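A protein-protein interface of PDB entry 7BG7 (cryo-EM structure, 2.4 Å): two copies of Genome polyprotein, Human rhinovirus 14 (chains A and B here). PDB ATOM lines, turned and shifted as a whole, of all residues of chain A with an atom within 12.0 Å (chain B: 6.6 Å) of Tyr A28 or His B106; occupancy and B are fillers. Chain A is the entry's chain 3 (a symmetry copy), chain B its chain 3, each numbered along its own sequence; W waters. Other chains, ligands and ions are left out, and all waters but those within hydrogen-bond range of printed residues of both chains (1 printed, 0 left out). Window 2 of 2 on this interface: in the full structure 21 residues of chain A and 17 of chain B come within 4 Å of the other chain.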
ATOM      1  N   PRO A  22     -25.936 -19.750  19.774  1.00  0.00           N
ATOM      2  CA  PRO A  22     -25.102 -18.941  18.883  1.00  0.00           C
ATOM      3  C   PRO A  22     -25.677 -17.548  18.691  1.00  0.00           C
ATOM      4  O   PRO A  22     -26.891 -17.342  18.670  1.00  0.00           O
ATOM      5  CB  PRO A  22     -25.111 -19.733  17.572  1.00  0.00           C
ATOM      6  CG  PRO A  22     -26.363 -20.524  17.632  1.00  0.00           C
ATOM      7  CD  PRO A  22     -26.577 -20.865  19.061  1.00  0.00           C
ATOM      8  N   SER A  23     -24.778 -16.588  18.537  1.00  0.00           N
ATOM      9  CA  SER A  23     -25.163 -15.202  18.344  1.00  0.00           C
ATOM     10  C   SER A  23     -25.401 -14.911  16.867  1.00  0.00           C
ATOM     11  O   SER A  23     -24.641 -15.352  16.004  1.00  0.00           O
ATOM     12  CB  SER A  23     -24.071 -14.283  18.892  1.00  0.00           C
ATOM     13  OG  SER A  23     -24.469 -12.929  18.868  1.00  0.00           O
ATOM     14  N   ALA A  24     -26.460 -14.159  16.588  1.00  0.00           N
ATOM     15  CA  ALA A  24     -26.771 -13.764  15.222  1.00  0.00           C
ATOM     16  C   ALA A  24     -25.970 -12.544  14.794  1.00  0.00           C
ATOM     17  O   ALA A  24     -25.856 -12.277  13.596  1.00  0.00           O
ATOM     18  CB  ALA A  24     -28.264 -13.478  15.079  1.00  0.00           C
ATOM     19  N   LEU A  25     -25.419 -11.799  15.750  1.00  0.00           N
ATOM     20  CA  LEU A  25     -24.613 -10.615  15.485  1.00  0.00           C
ATOM     21  C   LEU A  25     -23.232 -10.827  16.088  1.00  0.00           C
ATOM     22  O   LEU A  25     -22.894 -10.233  17.121  1.00  0.00           O
ATOM     23  CB  LEU A  25     -25.264  -9.368  16.075  1.00  0.00           C
ATOM     24  CG  LEU A  25     -26.673  -9.046  15.590  1.00  0.00           C
ATOM     25  CD1 LEU A  25     -27.178  -7.772  16.245  1.00  0.00           C
ATOM     26  CD2 LEU A  25     -26.699  -8.928  14.084  1.00  0.00           C
ATOM     27  N   PRO A  26     -22.406 -11.664  15.466  1.00  0.00           N
ATOM     28  CA  PRO A  26     -21.061 -11.884  15.997  1.00  0.00           C
ATOM     29  C   PRO A  26     -20.252 -10.602  15.944  1.00  0.00           C
ATOM     30  O   PRO A  26     -20.371  -9.808  15.009  1.00  0.00           O
ATOM     31  CB  PRO A  26     -20.485 -12.965  15.075  1.00  0.00           C
ATOM     32  CG  PRO A  26     -21.281 -12.870  13.836  1.00  0.00           C
ATOM     33  CD  PRO A  26     -22.648 -12.444  14.242  1.00  0.00           C
ATOM     34  N   ASN A  27     -19.465 -10.379  16.993  1.00  0.00           N
ATOM     35  CA  ASN A  27     -18.512  -9.287  17.104  1.00  0.00           C
ATOM     36  C   ASN A  27     -19.203  -7.962  17.387  1.00  0.00           C
ATOM     37  O   ASN A  27     -18.540  -6.921  17.370  1.00  0.00           O
ATOM     38  CB  ASN A  27     -17.641  -9.158  15.853  1.00  0.00           C
ATOM     39  CG  ASN A  27     -16.791 -10.378  15.630  1.00  0.00           C
ATOM     40  OD1 ASN A  27     -15.880 -10.661  16.403  1.00  0.00           O
ATOM     41  ND2 ASN A  27     -17.079 -11.114  14.569  1.00  0.00           N
ATOM     42  N   TYR A  28     -20.508  -7.968  17.631  1.00  0.00           N
ATOM     43  CA  TYR A  28     -21.231  -6.747  17.950  1.00  0.00           C
ATOM     44  C   TYR A  28     -20.827  -6.258  19.333  1.00  0.00           C
ATOM     45  O   TYR A  28     -20.711  -7.046  20.272  1.00  0.00           O
ATOM     46  CB  TYR A  28     -22.740  -6.978  17.890  1.00  0.00           C
ATOM     47  CG  TYR A  28     -23.544  -5.770  18.299  1.00  0.00           C
ATOM     48  CD1 TYR A  28     -23.948  -4.830  17.364  1.00  0.00           C
ATOM     49  CD2 TYR A  28     -23.882  -5.561  19.627  1.00  0.00           C
ATOM     50  CE1 TYR A  28     -24.671  -3.724  17.741  1.00  0.00           C
ATOM     51  CE2 TYR A  28     -24.611  -4.463  20.010  1.00  0.00           C
ATOM     52  CZ  TYR A  28     -25.001  -3.548  19.063  1.00  0.00           C
ATOM     53  OH  TYR A  28     -25.720  -2.449  19.447  1.00  0.00           O
ATOM     54  N   GLU A  29     -20.580  -4.962  19.446  1.00  0.00           N
ATOM     55  CA  GLU A  29     -20.194  -4.341  20.707  1.00  0.00           C
ATOM     56  C   GLU A  29     -21.332  -3.468  21.214  1.00  0.00           C
ATOM     57  O   GLU A  29     -21.603  -2.407  20.630  1.00  0.00           O
ATOM     58  CB  GLU A  29     -18.916  -3.525  20.524  1.00  0.00           C
ATOM     59  CG  GLU A  29     -17.730  -4.392  20.131  1.00  0.00           C
ATOM     60  CD  GLU A  29     -16.435  -3.622  20.001  1.00  0.00           C
ATOM     61  OE1 GLU A  29     -16.215  -2.984  18.956  1.00  0.00           O
ATOM     62  OE2 GLU A  29     -15.644  -3.631  20.963  1.00  0.00           O
ATOM     63  N   PRO A  30     -22.048  -3.882  22.256  1.00  0.00           N
ATOM     64  CA  PRO A  30     -23.176  -3.083  22.749  1.00  0.00           C
ATOM     65  C   PRO A  30     -22.734  -1.804  23.440  1.00  0.00           C
ATOM     66  O   PRO A  30     -21.613  -1.679  23.931  1.00  0.00           O
ATOM     67  CB  PRO A  30     -23.873  -4.029  23.726  1.00  0.00           C
ATOM     68  CG  PRO A  30     -22.813  -4.935  24.185  1.00  0.00           C
ATOM     69  CD  PRO A  30     -21.866  -5.112  23.043  1.00  0.00           C
ATOM     70  N   THR A  31     -23.644  -0.838  23.449  1.00  0.00           N
ATOM     71  CA  THR A  31     -23.383   0.444  24.084  1.00  0.00           C
ATOM     72  C   THR A  31     -22.890   0.223  25.511  1.00  0.00           C
ATOM     73  O   THR A  31     -23.460  -0.597  26.239  1.00  0.00           O
ATOM     74  CB  THR A  31     -24.653   1.299  24.111  1.00  0.00           C
ATOM     75  OG1 THR A  31     -25.083   1.561  22.776  1.00  0.00           O
ATOM     76  CG2 THR A  31     -24.397   2.638  24.801  1.00  0.00           C
ATOM     77  N   PRO A  32     -21.862   0.941  25.954  1.00  0.00           N
ATOM     78  CA  PRO A  32     -21.392   0.762  27.329  1.00  0.00           C
ATOM     79  C   PRO A  32     -22.472   1.113  28.338  1.00  0.00           C
ATOM     80  O   PRO A  32     -23.368   1.913  28.074  1.00  0.00           O
ATOM     81  CB  PRO A  32     -20.192   1.713  27.424  1.00  0.00           C
ATOM     82  CG  PRO A  32     -20.394   2.691  26.344  1.00  0.00           C
ATOM     83  CD  PRO A  32     -21.059   1.943  25.240  1.00  0.00           C
ATOM     84  N   ARG A  33     -22.382   0.477  29.497  1.00  0.00           N
ATOM     85  CA  ARG A  33     -23.314   0.710  30.586  1.00  0.00           C
ATOM     86  C   ARG A  33     -22.911   1.968  31.340  1.00  0.00           C
ATOM     87  O   ARG A  33     -21.800   2.051  31.871  1.00  0.00           O
ATOM     88  CB  ARG A  33     -23.328  -0.489  31.529  1.00  0.00           C
ATOM     89  CG  ARG A  33     -23.898  -1.742  30.917  1.00  0.00           C
ATOM     90  CD  ARG A  33     -23.473  -2.985  31.669  1.00  0.00           C
ATOM     91  NE  ARG A  33     -24.289  -4.128  31.283  1.00  0.00           N
ATOM     92  CZ  ARG A  33     -24.047  -4.912  30.238  1.00  0.00           C
ATOM     93  NH1 ARG A  33     -22.996  -4.692  29.458  1.00  0.00           N
ATOM     94  NH2 ARG A  33     -24.867  -5.919  29.973  1.00  0.00           N
ATOM     95  N   VAL B 101     -20.169   3.241   5.523  1.00  0.00           N
ATOM     96  CA  VAL B 101     -21.144   3.484   6.580  1.00  0.00           C
ATOM     97  C   VAL B 101     -22.452   2.767   6.279  1.00  0.00           C
ATOM     98  O   VAL B 101     -23.162   2.347   7.197  1.00  0.00           O
ATOM     99  CB  VAL B 101     -21.341   5.001   6.766  1.00  0.00           C
ATOM    100  CG1 VAL B 101     -22.743   5.328   7.221  1.00  0.00           C
ATOM    101  CG2 VAL B 101     -20.337   5.530   7.766  1.00  0.00           C
ATOM    102  N   TYR B 104     -23.295  -0.696   7.779  1.00  0.00           N
ATOM    103  CA  TYR B 104     -23.553  -0.782   9.201  1.00  0.00           C
ATOM    104  C   TYR B 104     -24.769   0.062   9.527  1.00  0.00           C
ATOM    105  O   TYR B 104     -25.196   0.899   8.732  1.00  0.00           O
ATOM    106  CB  TYR B 104     -22.341  -0.327  10.024  1.00  0.00           C
ATOM    107  CG  TYR B 104     -21.139  -1.211   9.815  1.00  0.00           C
ATOM    108  CD1 TYR B 104     -20.869  -2.252  10.686  1.00  0.00           C
ATOM    109  CD2 TYR B 104     -20.287  -1.019   8.741  1.00  0.00           C
ATOM    110  CE1 TYR B 104     -19.785  -3.069  10.500  1.00  0.00           C
ATOM    111  CE2 TYR B 104     -19.193  -1.832   8.548  1.00  0.00           C
ATOM    112  CZ  TYR B 104     -18.948  -2.856   9.429  1.00  0.00           C
ATOM    113  OH  TYR B 104     -17.866  -3.676   9.248  1.00  0.00           O
ATOM    114  N   THR B 105     -25.361  -0.207  10.683  1.00  0.00           N
ATOM    115  CA  THR B 105     -26.608   0.427  11.084  1.00  0.00           C
ATOM    116  C   THR B 105     -26.378   1.601  12.019  1.00  0.00           C
ATOM    117  O   THR B 105     -27.100   2.592  11.945  1.00  0.00           O
ATOM    118  CB  THR B 105     -27.527  -0.591  11.770  1.00  0.00           C
ATOM    119  OG1 THR B 105     -27.593  -1.786  10.988  1.00  0.00           O
ATOM    120  CG2 THR B 105     -28.922  -0.035  11.938  1.00  0.00           C
ATOM    121  N   HIS B 106     -25.393   1.499  12.905  1.00  0.00           N
ATOM    122  CA  HIS B 106     -25.092   2.519  13.896  1.00  0.00           C
ATOM    123  C   HIS B 106     -23.723   3.125  13.636  1.00  0.00           C
ATOM    124  O   HIS B 106     -22.801   2.449  13.178  1.00  0.00           O
ATOM    125  CB  HIS B 106     -25.100   1.965  15.322  1.00  0.00           C
ATOM    126  CG  HIS B 106     -26.335   1.207  15.685  1.00  0.00           C
ATOM    127  ND1 HIS B 106     -26.323   0.164  16.582  1.00  0.00           N
ATOM    128  CD2 HIS B 106     -27.620   1.351  15.292  1.00  0.00           C
ATOM    129  CE1 HIS B 106     -27.548  -0.303  16.725  1.00  0.00           C
ATOM    130  NE2 HIS B 106     -28.351   0.393  15.945  1.00  0.00           N
ATOM    131  N   TRP B 107     -23.592   4.407  13.948  1.00  0.00           N
ATOM    132  CA  TRP B 107     -22.308   5.076  13.873  1.00  0.00           C
ATOM    133  C   TRP B 107     -22.172   6.087  14.998  1.00  0.00           C
ATOM    134  O   TRP B 107     -23.146   6.708  15.424  1.00  0.00           O
ATOM    135  CB  TRP B 107     -22.112   5.752  12.513  1.00  0.00           C
ATOM    136  CG  TRP B 107     -22.811   7.059  12.344  1.00  0.00           C
ATOM    137  CD1 TRP B 107     -24.089   7.254  11.930  1.00  0.00           C
ATOM    138  CD2 TRP B 107     -22.259   8.360  12.569  1.00  0.00           C
ATOM    139  NE1 TRP B 107     -24.373   8.592  11.884  1.00  0.00           N
ATOM    140  CE2 TRP B 107     -23.267   9.295  12.278  1.00  0.00           C
ATOM    141  CE3 TRP B 107     -21.017   8.824  12.999  1.00  0.00           C
ATOM    142  CZ2 TRP B 107     -23.068  10.666  12.391  1.00  0.00           C
ATOM    143  CZ3 TRP B 107     -20.820  10.184  13.112  1.00  0.00           C
ATOM    144  CH2 TRP B 107     -21.838  11.089  12.811  1.00  0.00           C
ATOM    145  N   SER B 108     -20.943   6.234  15.478  1.00  0.00           N
ATOM    146  CA  SER B 108     -20.608   7.252  16.457  1.00  0.00           C
ATOM    147  C   SER B 108     -19.228   7.783  16.111  1.00  0.00           C
ATOM    148  O   SER B 108     -18.471   7.152  15.373  1.00  0.00           O
ATOM    149  CB  SER B 108     -20.650   6.696  17.888  1.00  0.00           C
ATOM    150  OG  SER B 108     -20.239   7.659  18.833  1.00  0.00           O
ATOM    151  N   PHE B 173     -24.996   6.413  20.103  1.00  0.00           N
ATOM    152  CA  PHE B 173     -24.880   5.997  18.716  1.00  0.00           C
ATOM    153  C   PHE B 173     -26.027   6.576  17.908  1.00  0.00           C
ATOM    154  O   PHE B 173     -27.142   6.745  18.400  1.00  0.00           O
ATOM    155  CB  PHE B 173     -24.864   4.470  18.574  1.00  0.00           C
ATOM    156  CG  PHE B 173     -23.574   3.842  19.000  1.00  0.00           C
ATOM    157  CD1 PHE B 173     -22.578   3.578  18.078  1.00  0.00           C
ATOM    158  CD2 PHE B 173     -23.340   3.553  20.327  1.00  0.00           C
ATOM    159  CE1 PHE B 173     -21.393   3.013  18.470  1.00  0.00           C
ATOM    160  CE2 PHE B 173     -22.156   2.996  20.724  1.00  0.00           C
ATOM    161  CZ  PHE B 173     -21.178   2.725  19.797  1.00  0.00           C
ATOM    162  N   ARG B 174     -25.724   6.907  16.663  1.00  0.00           N
ATOM    163  CA  ARG B 174     -26.706   7.405  15.721  1.00  0.00           C
ATOM    164  C   ARG B 174     -26.941   6.365  14.637  1.00  0.00           C
ATOM    165  O   ARG B 174     -26.078   5.535  14.354  1.00  0.00           O
ATOM    166  CB  ARG B 174     -26.248   8.724  15.090  1.00  0.00           C
ATOM    167  CG  ARG B 174     -26.477   9.939  15.971  1.00  0.00           C
ATOM    168  CD  ARG B 174     -26.398  11.231  15.174  1.00  0.00           C
ATOM    169  NE  ARG B 174     -25.099  11.890  15.196  1.00  0.00           N
ATOM    170  CZ  ARG B 174     -24.819  12.992  15.885  1.00  0.00           C
ATOM    171  NH1 ARG B 174     -25.742  13.593  16.622  1.00  0.00           N
ATOM    172  NH2 ARG B 174     -23.607  13.509  15.816  1.00  0.00           N
ATOM    173  N   TYR B 175     -28.116   6.424  14.026  1.00  0.00           N
ATOM    174  CA  TYR B 175     -28.427   5.536  12.921  1.00  0.00           C
ATOM    175  C   TYR B 175     -27.774   6.044  11.647  1.00  0.00           C
ATOM    176  O   TYR B 175     -27.772   7.243  11.370  1.00  0.00           O
ATOM    177  CB  TYR B 175     -29.938   5.437  12.712  1.00  0.00           C
ATOM    178  CG  TYR B 175     -30.671   4.598  13.724  1.00  0.00           C
ATOM    179  CD1 TYR B 175     -30.319   3.275  13.937  1.00  0.00           C
ATOM    180  CD2 TYR B 175     -31.713   5.124  14.467  1.00  0.00           C
ATOM    181  CE1 TYR B 175     -30.984   2.502  14.853  1.00  0.00           C
ATOM    182  CE2 TYR B 175     -32.380   4.361  15.391  1.00  0.00           C
ATOM    183  CZ  TYR B 175     -32.013   3.044  15.577  1.00  0.00           C
ATOM    184  OH  TYR B 175     -32.669   2.269  16.492  1.00  0.00           O
ATOM    185  N   THR B 176     -27.213   5.120  10.872  1.00  0.00           N
ATOM    186  CA  THR B 176     -26.575   5.510   9.621  1.00  0.00           C
ATOM    187  C   THR B 176     -27.618   5.972   8.612  1.00  0.00           C
ATOM    188  O   THR B 176     -27.316   6.798   7.747  1.00  0.00           O
ATOM    189  CB  THR B 176     -25.737   4.365   9.047  1.00  0.00           C
ATOM    190  OG1 THR B 176     -26.550   3.208   8.853  1.00  0.00           O
ATOM    191  CG2 THR B 176     -24.590   4.026   9.978  1.00  0.00           C
ATOM    192  N   PHE B 217     -13.930   6.998  15.511  1.00  0.00           N
ATOM    193  CA  PHE B 217     -15.128   6.590  14.801  1.00  0.00           C
ATOM    194  C   PHE B 217     -15.511   5.150  15.136  1.00  0.00           C
ATOM    195  O   PHE B 217     -14.655   4.292  15.357  1.00  0.00           O
ATOM    196  CB  PHE B 217     -14.909   6.737  13.299  1.00  0.00           C
ATOM    197  CG  PHE B 217     -16.161   6.962  12.530  1.00  0.00           C
ATOM    198  CD1 PHE B 217     -16.778   8.195  12.537  1.00  0.00           C
ATOM    199  CD2 PHE B 217     -16.724   5.946  11.792  1.00  0.00           C
ATOM    200  CE1 PHE B 217     -17.930   8.404  11.829  1.00  0.00           C
ATOM    201  CE2 PHE B 217     -17.876   6.154  11.083  1.00  0.00           C
ATOM    202  CZ  PHE B 217     -18.481   7.382  11.100  1.00  0.00           C
ATOM    203  N   LYS B 218     -16.815   4.892  15.148  1.00  0.00           N
ATOM    204  CA  LYS B 218     -17.357   3.588  15.496  1.00  0.00           C
ATOM    205  C   LYS B 218     -18.451   3.209  14.511  1.00  0.00           C
ATOM    206  O   LYS B 218     -19.245   4.057  14.101  1.00  0.00           O
ATOM    207  CB  LYS B 218     -17.946   3.579  16.916  1.00  0.00           C
ATOM    208  CG  LYS B 218     -17.022   4.067  18.008  1.00  0.00           C
ATOM    209  CD  LYS B 218     -17.728   4.087  19.351  1.00  0.00           C
ATOM    210  CE  LYS B 218     -17.037   4.979  20.355  1.00  0.00           C
ATOM    211  NZ  LYS B 218     -17.102   6.412  19.968  1.00  0.00           N
ATOM    212  N   LEU B 219     -18.496   1.931  14.146  1.00  0.00           N
ATOM    213  CA  LEU B 219     -19.572   1.377  13.334  1.00  0.00           C
ATOM    214  C   LEU B 219     -19.931   0.008  13.875  1.00  0.00           C
ATOM    215  O   LEU B 219     -19.040  -0.815  14.096  1.00  0.00           O
ATOM    216  CB  LEU B 219     -19.169   1.249  11.864  1.00  0.00           C
ATOM    217  CG  LEU B 219     -18.859   2.527  11.094  1.00  0.00           C
ATOM    218  CD1 LEU B 219     -18.275   2.181   9.736  1.00  0.00           C
ATOM    219  CD2 LEU B 219     -20.105   3.370  10.960  1.00  0.00           C
ATOM    220  N   ARG B 220     -21.213  -0.221  14.159  1.00  0.00           N
ATOM    221  CA  ARG B 220     -21.601  -1.389  14.941  1.00  0.00           C
ATOM    222  C   ARG B 220     -22.278  -2.476  14.117  1.00  0.00           C
ATOM    223  O   ARG B 220     -21.662  -3.497  13.837  1.00  0.00           O
ATOM    224  CB  ARG B 220     -22.507  -0.981  16.097  1.00  0.00           C
ATOM    225  CG  ARG B 220     -21.796  -0.252  17.187  1.00  0.00           C
ATOM    226  CD  ARG B 220     -22.497  -0.451  18.496  1.00  0.00           C
ATOM    227  NE  ARG B 220     -23.845   0.095  18.485  1.00  0.00           N
ATOM    228  CZ  ARG B 220     -24.534   0.370  19.582  1.00  0.00           C
ATOM    229  NH1 ARG B 220     -23.995   0.155  20.771  1.00  0.00           N
ATOM    230  NH2 ARG B 220     -25.754   0.867  19.498  1.00  0.00           N
ATOM    231  N   LEU B 221     -23.492  -2.262  13.648  1.00  0.00           N
ATOM    232  CA  LEU B 221     -24.389  -3.369  13.320  1.00  0.00           C
ATOM    233  C   LEU B 221     -24.450  -3.558  11.808  1.00  0.00           C
ATOM    234  O   LEU B 221     -25.021  -2.732  11.094  1.00  0.00           O
ATOM    235  CB  LEU B 221     -25.766  -3.118  13.931  1.00  0.00           C
ATOM    236  CG  LEU B 221     -26.911  -4.107  13.716  1.00  0.00           C
ATOM    237  CD1 LEU B 221     -26.428  -5.527  13.684  1.00  0.00           C
ATOM    238  CD2 LEU B 221     -27.922  -3.916  14.830  1.00  0.00           C
ATOM    239  N   MET B 222     -23.884  -4.666  11.335  1.00  0.00           N
ATOM    240  CA  MET B 222     -23.763  -4.924   9.907  1.00  0.00           C
ATOM    241  C   MET B 222     -25.127  -5.060   9.254  1.00  0.00           C
ATOM    242  O   MET B 222     -26.048  -5.671   9.802  1.00  0.00           O
ATOM    243  CB  MET B 222     -22.968  -6.201   9.659  1.00  0.00           C
ATOM    244  CG  MET B 222     -21.514  -6.112  10.027  1.00  0.00           C
ATOM    245  SD  MET B 222     -20.444  -7.034   8.912  1.00  0.00           S
ATOM    246  CE  MET B 222     -20.986  -8.699   9.258  1.00  0.00           C
HETATM  247  O   HOH W   1     -26.102  -1.839  22.027  1.00  0.00           O
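NH1 of Arg B220 sits at hydrogen-bond distance from OG1 of Thr A31, at 2.7 Å. The guanidinium group of Arg B220 lies close to the side-chain hydroxyl of Tyr A28.
Water W1 lies within hydrogen-bond range of OH of Tyr A28 (2.7 Å), N of Thr A31 (3.0 Å) and NH1 of Arg B220 (3.2 Å).
No position is printed for both chains.
N of Thr B105 lies within hydrogen-bond range of O of Leu B221 (2.6 Å). NH2 of Arg B220 lies within hydrogen-bond range of ND1 of His B106 (3.1 Å). OG of Ser A23 lies close to N of Leu A25.
Printed residues of chain B within 4 Å of Tyr A28: His B106 and Arg B220. Of the printed residues of chain B, Glu A29 touches Arg B220. Printed residues of chain B within 4 Å of Pro A30: Arg B220. No residue of chain A comes within 4 Å of Thr B105. Printed residues of chain A within 4 Å of His B106: Tyr A28 (3.9 Å). No residue of chain A comes within 4 Å of Ser B108. Phe B173 touches just one residue of chain A: Thr A31 (3.6 Å). No residue of chain A comes within 4 Å of Tyr B175. No residue of chain A comes within 4 Å of Leu B219. Arg B220 touches four residues of chain A. The nearest printed residue of chain B that does not touch Tyr A28 is Leu B221 (4.01 Å). The nearest printed residue of chain B that does not touch Glu A29 is Phe B173 (5.2 Å).
Of the 16 printed residues of chain B, 4 touch a printed residue of chain A. Printed residues of chain B that touch a printed residue of chain A: His B106, Phe B173, Arg B220 and Leu B221. Along chain B the printed residues that touch a printed residue of chain A span positions 106 to 221. Of the 12 printed residues of chain A, 5 touch a printed residue of chain B. Hydrophobic or aromatic side chains of chain A within 4 Å of the printed part of chain B: Leu A25 and Tyr A28. Along chain A the printed residues that touch a printed residue of chain B span positions 25 to 31. Among the printed residues, 7 pairs touch across the chains. Among the printed residues, no Asp or Glu carboxylate lies within 4 Å of a Lys or Arg side-chain nitrogen of the other chain.
Leu A25 touches Leu B221 (CD2 to CD1, 3.4 Å). His B106 touches Tyr A28 (CE1 to OH, 3.9 Å). O of Glu A29 touches CD of Arg B220 (3.0 Å). NH1 of Arg B220 touches C of Pro A30, 3.5 Å away. Thr A31 touches Phe B173 (OG1 to CD2, 3.6 Å).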
